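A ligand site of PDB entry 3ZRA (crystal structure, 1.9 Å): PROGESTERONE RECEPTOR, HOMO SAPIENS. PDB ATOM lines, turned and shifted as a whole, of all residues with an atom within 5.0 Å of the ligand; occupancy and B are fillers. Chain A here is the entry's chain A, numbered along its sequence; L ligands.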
ATOM      1  N   LEU A  42      21.499  10.988 -21.063  1.00  0.00           N
ATOM      2  CA  LEU A  42      20.299  11.166 -21.881  1.00  0.00           C
ATOM      3  C   LEU A  42      20.233  12.584 -22.457  1.00  0.00           C
ATOM      4  O   LEU A  42      19.904  12.758 -23.618  1.00  0.00           O
ATOM      5  CB  LEU A  42      19.037  10.841 -21.085  1.00  0.00           C
ATOM      6  CG  LEU A  42      18.871   9.340 -20.785  1.00  0.00           C
ATOM      7  CD1 LEU A  42      17.880   9.120 -19.643  1.00  0.00           C
ATOM      8  CD2 LEU A  42      18.435   8.565 -22.010  1.00  0.00           C
ATOM      9  N   THR A  43      20.597  13.582 -21.647  1.00  0.00           N
ATOM     10  CA  THR A  43      20.690  14.956 -22.142  1.00  0.00           C
ATOM     11  C   THR A  43      21.692  15.090 -23.292  1.00  0.00           C
ATOM     12  O   THR A  43      21.378  15.719 -24.300  1.00  0.00           O
ATOM     13  CB  THR A  43      21.058  15.941 -21.030  1.00  0.00           C
ATOM     14  OG1 THR A  43      20.079  15.885 -19.979  1.00  0.00           O
ATOM     15  CG2 THR A  43      21.110  17.378 -21.581  1.00  0.00           C
ATOM     16  N   LEU A  45      22.794  12.746 -25.307  1.00  0.00           N
ATOM     17  CA  LEU A  45      22.265  12.013 -26.458  1.00  0.00           C
ATOM     18  C   LEU A  45      21.188  12.815 -27.198  1.00  0.00           C
ATOM     19  O   LEU A  45      21.160  12.820 -28.417  1.00  0.00           O
ATOM     20  CB  LEU A  45      21.748  10.619 -26.051  1.00  0.00           C
ATOM     21  CG  LEU A  45      22.844   9.610 -25.690  1.00  0.00           C
ATOM     22  CD1 LEU A  45      22.262   8.338 -25.078  1.00  0.00           C
ATOM     23  CD2 LEU A  45      23.700   9.268 -26.904  1.00  0.00           C
ATOM     24  N   ASN A  46      20.321  13.517 -26.460  1.00  0.00           N
ATOM     25  CA  ASN A  46      19.319  14.374 -27.109  1.00  0.00           C
ATOM     26  C   ASN A  46      19.927  15.576 -27.821  1.00  0.00           C
ATOM     27  O   ASN A  46      19.450  15.970 -28.880  1.00  0.00           O
ATOM     28  CB  ASN A  46      18.230  14.840 -26.129  1.00  0.00           C
ATOM     29  CG  ASN A  46      17.117  13.816 -25.943  1.00  0.00           C
ATOM     30  OD1 ASN A  46      17.028  12.848 -26.694  1.00  0.00           O
ATOM     31  ND2 ASN A  46      16.251  14.034 -24.947  1.00  0.00           N
ATOM     32  N   LEU A  48      23.011  15.668 -29.065  1.00  0.00           N
ATOM     33  CA  LEU A  48      23.585  15.029 -30.245  1.00  0.00           C
ATOM     34  C   LEU A  48      22.478  14.793 -31.267  1.00  0.00           C
ATOM     35  O   LEU A  48      22.625  15.133 -32.443  1.00  0.00           O
ATOM     36  CB  LEU A  48      24.271  13.705 -29.857  1.00  0.00           C
ATOM     37  CG  LEU A  48      24.912  12.881 -30.976  1.00  0.00           C
ATOM     38  CD1 LEU A  48      26.026  13.663 -31.662  1.00  0.00           C
ATOM     39  CD2 LEU A  48      25.437  11.551 -30.452  1.00  0.00           C
ATOM     40  N   GLY A  49      21.361  14.238 -30.806  1.00  0.00           N
ATOM     41  CA  GLY A  49      20.150  14.039 -31.610  1.00  0.00           C
ATOM     42  C   GLY A  49      19.715  15.284 -32.353  1.00  0.00           C
ATOM     43  O   GLY A  49      19.428  15.222 -33.548  1.00  0.00           O
ATOM     44  N   GLN A  52      22.401  16.042 -35.114  1.00  0.00           N
ATOM     45  CA  GLN A  52      22.241  15.072 -36.195  1.00  0.00           C
ATOM     46  C   GLN A  52      20.981  15.341 -37.021  1.00  0.00           C
ATOM     47  O   GLN A  52      21.007  15.139 -38.233  1.00  0.00           O
ATOM     48  CB  GLN A  52      22.215  13.653 -35.643  1.00  0.00           C
ATOM     49  CG  GLN A  52      23.587  13.272 -35.108  1.00  0.00           C
ATOM     50  CD  GLN A  52      23.668  11.837 -34.631  1.00  0.00           C
ATOM     51  OE1 GLN A  52      22.670  11.151 -34.512  1.00  0.00           O
ATOM     52  NE2 GLN A  52      24.885  11.400 -34.341  1.00  0.00           N
ATOM     53  N   TRP A  82      13.416  10.310 -39.337  1.00  0.00           N
ATOM     54  CA  TRP A  82      14.627  10.758 -38.616  1.00  0.00           C
ATOM     55  C   TRP A  82      15.192   9.697 -37.670  1.00  0.00           C
ATOM     56  O   TRP A  82      16.415   9.568 -37.558  1.00  0.00           O
ATOM     57  CB  TRP A  82      14.391  12.068 -37.846  1.00  0.00           C
ATOM     58  CG  TRP A  82      13.357  11.964 -36.754  1.00  0.00           C
ATOM     59  CD1 TRP A  82      12.009  12.120 -36.893  1.00  0.00           C
ATOM     60  CD2 TRP A  82      13.590  11.665 -35.367  1.00  0.00           C
ATOM     61  NE1 TRP A  82      11.380  11.923 -35.678  1.00  0.00           N
ATOM     62  CE2 TRP A  82      12.327  11.656 -34.720  1.00  0.00           C
ATOM     63  CE3 TRP A  82      14.734  11.407 -34.601  1.00  0.00           C
ATOM     64  CZ2 TRP A  82      12.174  11.407 -33.361  1.00  0.00           C
ATOM     65  CZ3 TRP A  82      14.590  11.157 -33.236  1.00  0.00           C
ATOM     66  CH2 TRP A  82      13.311  11.157 -32.636  1.00  0.00           C
ATOM     67  N   MET A  83      14.311   8.952 -37.005  1.00  0.00           N
ATOM     68  CA  MET A  83      14.742   7.958 -36.010  1.00  0.00           C
ATOM     69  C   MET A  83      15.421   6.786 -36.711  1.00  0.00           C
ATOM     70  O   MET A  83      16.445   6.282 -36.225  1.00  0.00           O
ATOM     71  CB  MET A  83      13.557   7.459 -35.167  1.00  0.00           C
ATOM     72  CG  MET A  83      13.909   6.329 -34.194  1.00  0.00           C
ATOM     73  SD  MET A  83      14.776   6.884 -32.718  1.00  0.00           S
ATOM     74  CE  MET A  83      13.403   7.737 -31.924  1.00  0.00           C
ATOM     75  N   MET A  86      18.851   8.032 -37.834  1.00  0.00           N
ATOM     76  CA  MET A  86      19.796   8.263 -36.748  1.00  0.00           C
ATOM     77  C   MET A  86      20.392   6.937 -36.242  1.00  0.00           C
ATOM     78  O   MET A  86      21.597   6.848 -35.989  1.00  0.00           O
ATOM     79  CB  MET A  86      19.158   9.081 -35.617  1.00  0.00           C
ATOM     80  CG  MET A  86      19.142  10.603 -35.891  1.00  0.00           C
ATOM     81  SD  MET A  86      18.499  11.657 -34.546  1.00  0.00           S
ATOM     82  CE  MET A  86      19.017  10.695 -33.132  1.00  0.00           C
ATOM     83  N   VAL A  87      19.562   5.900 -36.160  1.00  0.00           N
ATOM     84  CA  VAL A  87      20.020   4.596 -35.679  1.00  0.00           C
ATOM     85  C   VAL A  87      20.784   3.811 -36.742  1.00  0.00           C
ATOM     86  O   VAL A  87      21.645   2.980 -36.425  1.00  0.00           O
ATOM     87  CB  VAL A  87      18.852   3.760 -35.096  1.00  0.00           C
ATOM     88  CG1 VAL A  87      17.935   3.266 -36.215  1.00  0.00           C
ATOM     89  CG2 VAL A  87      19.393   2.595 -34.252  1.00  0.00           C
ATOM     90  N   LEU A  90      24.131   5.470 -36.508  1.00  0.00           N
ATOM     91  CA  LEU A  90      24.840   4.933 -35.342  1.00  0.00           C
ATOM     92  C   LEU A  90      25.423   3.577 -35.677  1.00  0.00           C
ATOM     93  O   LEU A  90      26.556   3.296 -35.353  1.00  0.00           O
ATOM     94  CB  LEU A  90      23.894   4.803 -34.150  1.00  0.00           C
ATOM     95  CG  LEU A  90      24.368   4.051 -32.904  1.00  0.00           C
ATOM     96  CD1 LEU A  90      25.489   4.812 -32.214  1.00  0.00           C
ATOM     97  CD2 LEU A  90      23.173   3.873 -31.975  1.00  0.00           C
ATOM     98  N   ARG A  93      28.630   4.133 -38.085  1.00  0.00           N
ATOM     99  CA  ARG A  93      29.762   4.637 -37.311  1.00  0.00           C
ATOM    100  C   ARG A  93      30.323   3.559 -36.379  1.00  0.00           C
ATOM    101  O   ARG A  93      31.537   3.386 -36.275  1.00  0.00           O
ATOM    102  CB  ARG A  93      29.386   5.869 -36.482  1.00  0.00           C
ATOM    103  CG  ARG A  93      29.134   7.121 -37.302  1.00  0.00           C
ATOM    104  CD  ARG A  93      28.996   8.372 -36.433  1.00  0.00           C
ATOM    105  NE  ARG A  93      27.938   8.262 -35.432  1.00  0.00           N
ATOM    106  CZ  ARG A  93      26.627   8.383 -35.667  1.00  0.00           C
ATOM    107  NH1 ARG A  93      26.156   8.623 -36.897  1.00  0.00           N
ATOM    108  NH2 ARG A  93      25.761   8.256 -34.668  1.00  0.00           N
ATOM    109  N   PHE A 105      28.209   6.804 -30.697  1.00  0.00           N
ATOM    110  CA  PHE A 105      27.264   7.896 -30.894  1.00  0.00           C
ATOM    111  C   PHE A 105      27.990   9.113 -31.458  1.00  0.00           C
ATOM    112  O   PHE A 105      27.476   9.809 -32.337  1.00  0.00           O
ATOM    113  CB  PHE A 105      26.538   8.257 -29.604  1.00  0.00           C
ATOM    114  CG  PHE A 105      25.649   7.163 -29.072  1.00  0.00           C
ATOM    115  CD1 PHE A 105      24.344   7.017 -29.527  1.00  0.00           C
ATOM    116  CD2 PHE A 105      26.114   6.282 -28.101  1.00  0.00           C
ATOM    117  CE1 PHE A 105      23.522   6.008 -29.015  1.00  0.00           C
ATOM    118  CE2 PHE A 105      25.289   5.278 -27.602  1.00  0.00           C
ATOM    119  CZ  PHE A 105      24.002   5.142 -28.066  1.00  0.00           C
ATOM    120  N   LEU A 124      17.626  -0.564 -24.076  1.00  0.00           N
ATOM    121  CA  LEU A 124      17.638   0.312 -25.247  1.00  0.00           C
ATOM    122  C   LEU A 124      18.963   0.187 -25.984  1.00  0.00           C
ATOM    123  O   LEU A 124      18.982   0.156 -27.223  1.00  0.00           O
ATOM    124  CB  LEU A 124      17.390   1.788 -24.862  1.00  0.00           C
ATOM    125  CG  LEU A 124      17.151   2.741 -26.044  1.00  0.00           C
ATOM    126  CD1 LEU A 124      15.798   2.504 -26.708  1.00  0.00           C
ATOM    127  CD2 LEU A 124      17.289   4.201 -25.609  1.00  0.00           C
ATOM    128  N   MET A 128      19.518  -1.055 -29.939  1.00  0.00           N
ATOM    129  CA  MET A 128      20.237  -0.231 -30.915  1.00  0.00           C
ATOM    130  C   MET A 128      21.468  -0.968 -31.464  1.00  0.00           C
ATOM    131  O   MET A 128      21.824  -0.809 -32.631  1.00  0.00           O
ATOM    132  CB  MET A 128      20.668   1.092 -30.284  1.00  0.00           C
ATOM    133  CG  MET A 128      19.523   2.072 -29.971  1.00  0.00           C
ATOM    134  SD  MET A 128      20.110   3.645 -29.298  1.00  0.00           S
ATOM    135  CE  MET A 128      20.704   3.170 -27.695  1.00  0.00           C
ATOM    136  N   LEU A 214      11.994   2.032 -30.564  1.00  0.00           N
ATOM    137  CA  LEU A 214      12.685   3.300 -30.263  1.00  0.00           C
ATOM    138  C   LEU A 214      11.687   4.452 -30.192  1.00  0.00           C
ATOM    139  O   LEU A 214      11.782   5.334 -29.314  1.00  0.00           O
ATOM    140  CB  LEU A 214      13.788   3.609 -31.294  1.00  0.00           C
ATOM    141  CG  LEU A 214      14.863   2.545 -31.546  1.00  0.00           C
ATOM    142  CD1 LEU A 214      15.908   3.014 -32.563  1.00  0.00           C
ATOM    143  CD2 LEU A 214      15.544   2.121 -30.252  1.00  0.00           C
ATOM    144  N   TYR A 217       9.860   4.185 -26.773  1.00  0.00           N
ATOM    145  CA  TYR A 217      10.796   4.645 -25.761  1.00  0.00           C
ATOM    146  C   TYR A 217      10.986   6.170 -25.819  1.00  0.00           C
ATOM    147  O   TYR A 217      11.049   6.840 -24.786  1.00  0.00           O
ATOM    148  CB  TYR A 217      12.150   3.932 -25.927  1.00  0.00           C
ATOM    149  CG  TYR A 217      13.123   4.190 -24.789  1.00  0.00           C
ATOM    150  CD1 TYR A 217      13.874   5.355 -24.755  1.00  0.00           C
ATOM    151  CD2 TYR A 217      13.286   3.271 -23.763  1.00  0.00           C
ATOM    152  CE1 TYR A 217      14.768   5.608 -23.718  1.00  0.00           C
ATOM    153  CE2 TYR A 217      14.179   3.502 -22.727  1.00  0.00           C
ATOM    154  CZ  TYR A 217      14.908   4.682 -22.712  1.00  0.00           C
ATOM    155  OH  TYR A 217      15.817   4.928 -21.697  1.00  0.00           O
ATOM    156  N   CYS A 218      11.053   6.693 -27.038  1.00  0.00           N
ATOM    157  CA  CYS A 218      11.183   8.131 -27.252  1.00  0.00           C
ATOM    158  C   CYS A 218       9.954   8.860 -26.708  1.00  0.00           C
ATOM    159  O   CYS A 218      10.081   9.830 -25.943  1.00  0.00           O
ATOM    160  CB  CYS A 218      11.381   8.447 -28.746  1.00  0.00           C
ATOM    161  SG  CYS A 218      11.234  10.216 -29.124  1.00  0.00           S
ATOM    162  N   THR A 221       9.824   8.707 -22.889  1.00  0.00           N
ATOM    163  CA  THR A 221      10.842   9.612 -22.356  1.00  0.00           C
ATOM    164  C   THR A 221      10.435  11.089 -22.514  1.00  0.00           C
ATOM    165  O   THR A 221      10.627  11.891 -21.609  1.00  0.00           O
ATOM    166  CB  THR A 221      12.238   9.363 -23.015  1.00  0.00           C
ATOM    167  OG1 THR A 221      12.660   8.009 -22.775  1.00  0.00           O
ATOM    168  CG2 THR A 221      13.294  10.326 -22.442  1.00  0.00           C
ATOM    169  N   VAL A 230      15.689  15.253 -18.424  1.00  0.00           N
ATOM    170  CA  VAL A 230      16.225  15.035 -19.777  1.00  0.00           C
ATOM    171  C   VAL A 230      15.586  16.044 -20.726  1.00  0.00           C
ATOM    172  O   VAL A 230      14.432  15.873 -21.121  1.00  0.00           O
ATOM    173  CB  VAL A 230      15.893  13.612 -20.295  1.00  0.00           C
ATOM    174  CG1 VAL A 230      16.560  13.361 -21.649  1.00  0.00           C
ATOM    175  CG2 VAL A 230      16.294  12.555 -19.280  1.00  0.00           C
ATOM    176  N   PHE A 232      14.636  18.098 -24.090  1.00  0.00           N
ATOM    177  CA  PHE A 232      14.445  17.861 -25.505  1.00  0.00           C
ATOM    178  C   PHE A 232      14.605  19.195 -26.232  1.00  0.00           C
ATOM    179  O   PHE A 232      13.802  20.091 -26.030  1.00  0.00           O
ATOM    180  CB  PHE A 232      13.064  17.263 -25.762  1.00  0.00           C
ATOM    181  CG  PHE A 232      12.977  15.800 -25.451  1.00  0.00           C
ATOM    182  CD1 PHE A 232      12.931  15.367 -24.127  1.00  0.00           C
ATOM    183  CD2 PHE A 232      12.997  14.861 -26.455  1.00  0.00           C
ATOM    184  CE1 PHE A 232      12.871  14.020 -23.829  1.00  0.00           C
ATOM    185  CE2 PHE A 232      12.937  13.514 -26.156  1.00  0.00           C
ATOM    186  CZ  PHE A 232      12.880  13.090 -24.834  1.00  0.00           C
ATOM    187  N   MET A 236      13.984  18.691 -32.411  1.00  0.00           N
ATOM    188  CA  MET A 236      13.572  17.356 -31.974  1.00  0.00           C
ATOM    189  C   MET A 236      12.167  17.365 -31.345  1.00  0.00           C
ATOM    190  O   MET A 236      11.322  16.529 -31.696  1.00  0.00           O
ATOM    191  CB  MET A 236      14.585  16.780 -30.985  1.00  0.00           C
ATOM    192  CG  MET A 236      14.218  15.395 -30.494  1.00  0.00           C
ATOM    193  SD  MET A 236      15.388  14.787 -29.291  1.00  0.00           S
ATOM    194  CE  MET A 236      16.839  14.606 -30.355  1.00  0.00           C
ATOM    195  N   ILE A 240       8.799  15.300 -32.960  1.00  0.00           N
ATOM    196  CA  ILE A 240       8.085  14.409 -32.054  1.00  0.00           C
ATOM    197  C   ILE A 240       6.621  14.818 -31.934  1.00  0.00           C
ATOM    198  O   ILE A 240       5.726  14.032 -32.203  1.00  0.00           O
ATOM    199  CB  ILE A 240       8.747  14.367 -30.639  1.00  0.00           C
ATOM    200  CG1 ILE A 240      10.067  13.639 -30.700  1.00  0.00           C
ATOM    201  CG2 ILE A 240       7.813  13.689 -29.630  1.00  0.00           C
ATOM    202  CD1 ILE A 240      10.984  13.843 -29.484  1.00  0.00           C
HETATM  203  F1  LIG L   1      20.009   5.367 -32.657  1.00  0.00           F
HETATM  204  C1  LIG L   1      20.443   6.511 -32.104  1.00  0.00           C
HETATM  205  C2  LIG L   1      19.809   6.947 -30.964  1.00  0.00           C
HETATM  206  C3  LIG L   1      20.251   8.129 -30.365  1.00  0.00           C
HETATM  207  C4  LIG L   1      21.321   8.829 -30.957  1.00  0.00           C
HETATM  208 CL1  LIG L   1      21.958  10.303 -30.315  1.00  0.00          CL
HETATM  209  N1  LIG L   1      21.887   8.364 -32.052  1.00  0.00           N
HETATM  210  C5  LIG L   1      21.493   7.251 -32.625  1.00  0.00           C
HETATM  211  C6  LIG L   1      19.518   8.538 -29.131  1.00  0.00           C
HETATM  212  C7  LIG L   1      19.258   7.573 -28.139  1.00  0.00           C
HETATM  213  C8  LIG L   1      18.562   7.907 -26.987  1.00  0.00           C
HETATM  214  C9  LIG L   1      18.140   9.213 -26.812  1.00  0.00           C
HETATM  215  C10 LIG L   1      18.395  10.173 -27.797  1.00  0.00           C
HETATM  216  C11 LIG L   1      19.067   9.841 -28.965  1.00  0.00           C
HETATM  217  C12 LIG L   1      17.383   9.605 -25.579  1.00  0.00           C
HETATM  218  C13 LIG L   1      18.232  10.568 -24.746  1.00  0.00           C
HETATM  219  N2  LIG L   1      16.134  10.283 -25.978  1.00  0.00           N
HETATM  220  S1  LIG L   1      14.854   9.474 -26.630  1.00  0.00           S
HETATM  221  O1  LIG L   1      14.754   8.247 -25.928  1.00  0.00           O
HETATM  222  O2  LIG L   1      13.777  10.402 -26.682  1.00  0.00           O
HETATM  223  C14 LIG L   1      15.329   9.095 -28.290  1.00  0.00           C
HETATM  224  C15 LIG L   1      15.540   9.969 -29.308  1.00  0.00           C
HETATM  225  C16 LIG L   1      15.349  11.456 -29.282  1.00  0.00           C
HETATM  226  O3  LIG L   1      15.941   9.245 -30.361  1.00  0.00           O
HETATM  227  N3  LIG L   1      15.984   8.055 -30.093  1.00  0.00           N
HETATM  228  C17 LIG L   1      15.650   7.832 -28.856  1.00  0.00           C
HETATM  229  C18 LIG L   1      15.629   6.486 -28.195  1.00  0.00           C
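N3 of the ligand lies close to SD of Met 83 (3.1 Å).
The side-chain sulfur (SD) of Met 128 lies close to a fluorine (F1) of the ligand (3.8 Å).
Residues that only touch the ligand: Leu 42 (3.0 Å), Leu 45 (3.3 Å), Leu 48 (3.7 Å), Gln 52 (3.8 Å), Trp 82 (3.7 Å), Met 86 (3.4 Å), Val 87 (3.1 Å), Leu 90 (3.6 Å), Phe 105 (3.8 Å), Leu 124 (3.8 Å), Tyr 217 (3.2 Å), Thr 221 (3.8 Å), Phe 232 (3.3 Å) and Met 236 (3.3 Å).
Hydrophobic or aromatic side chains that line the ligand: Leu 42, Leu 45, Leu 48, Trp 82, Met 83, Met 86, Val 87, Leu 90, Phe 105, Leu 124, Met 128, Tyr 217, Phe 232 and Met 236.
Within 4 Å of the ligand: Leu 42, Leu 45, Asn 46, Leu 48, Gln 52, Trp 82, Met 83, Met 86, Val 87, Leu 90, Phe 105, Leu 124, Met 128, Tyr 217, Cys 218, Thr 221, Phe 232 and Met 236.
The side-chain sulfur (SD) of Met 236 sits close to the side-chain amide oxygen (OD1) of Asn 46 (3.6 Å).
OG1 of Thr 221 is in hydrogen-bond range of O of Tyr 217.
The guanidinium group of Arg 93 is in hydrogen-bond range of the backbone carbonyl oxygen of Phe 105.
NE2 of Gln 52 sits close to NH2 of Arg 93 (3.3 Å).
The side-chain amide oxygen (OD1) of Asn 46 lies within hydrogen-bond range of a nitrogen (N2) of the ligand.
The side-chain sulfur (SG) of Cys 218 lies close to an oxygen (O2) of the ligand (3.5 Å).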
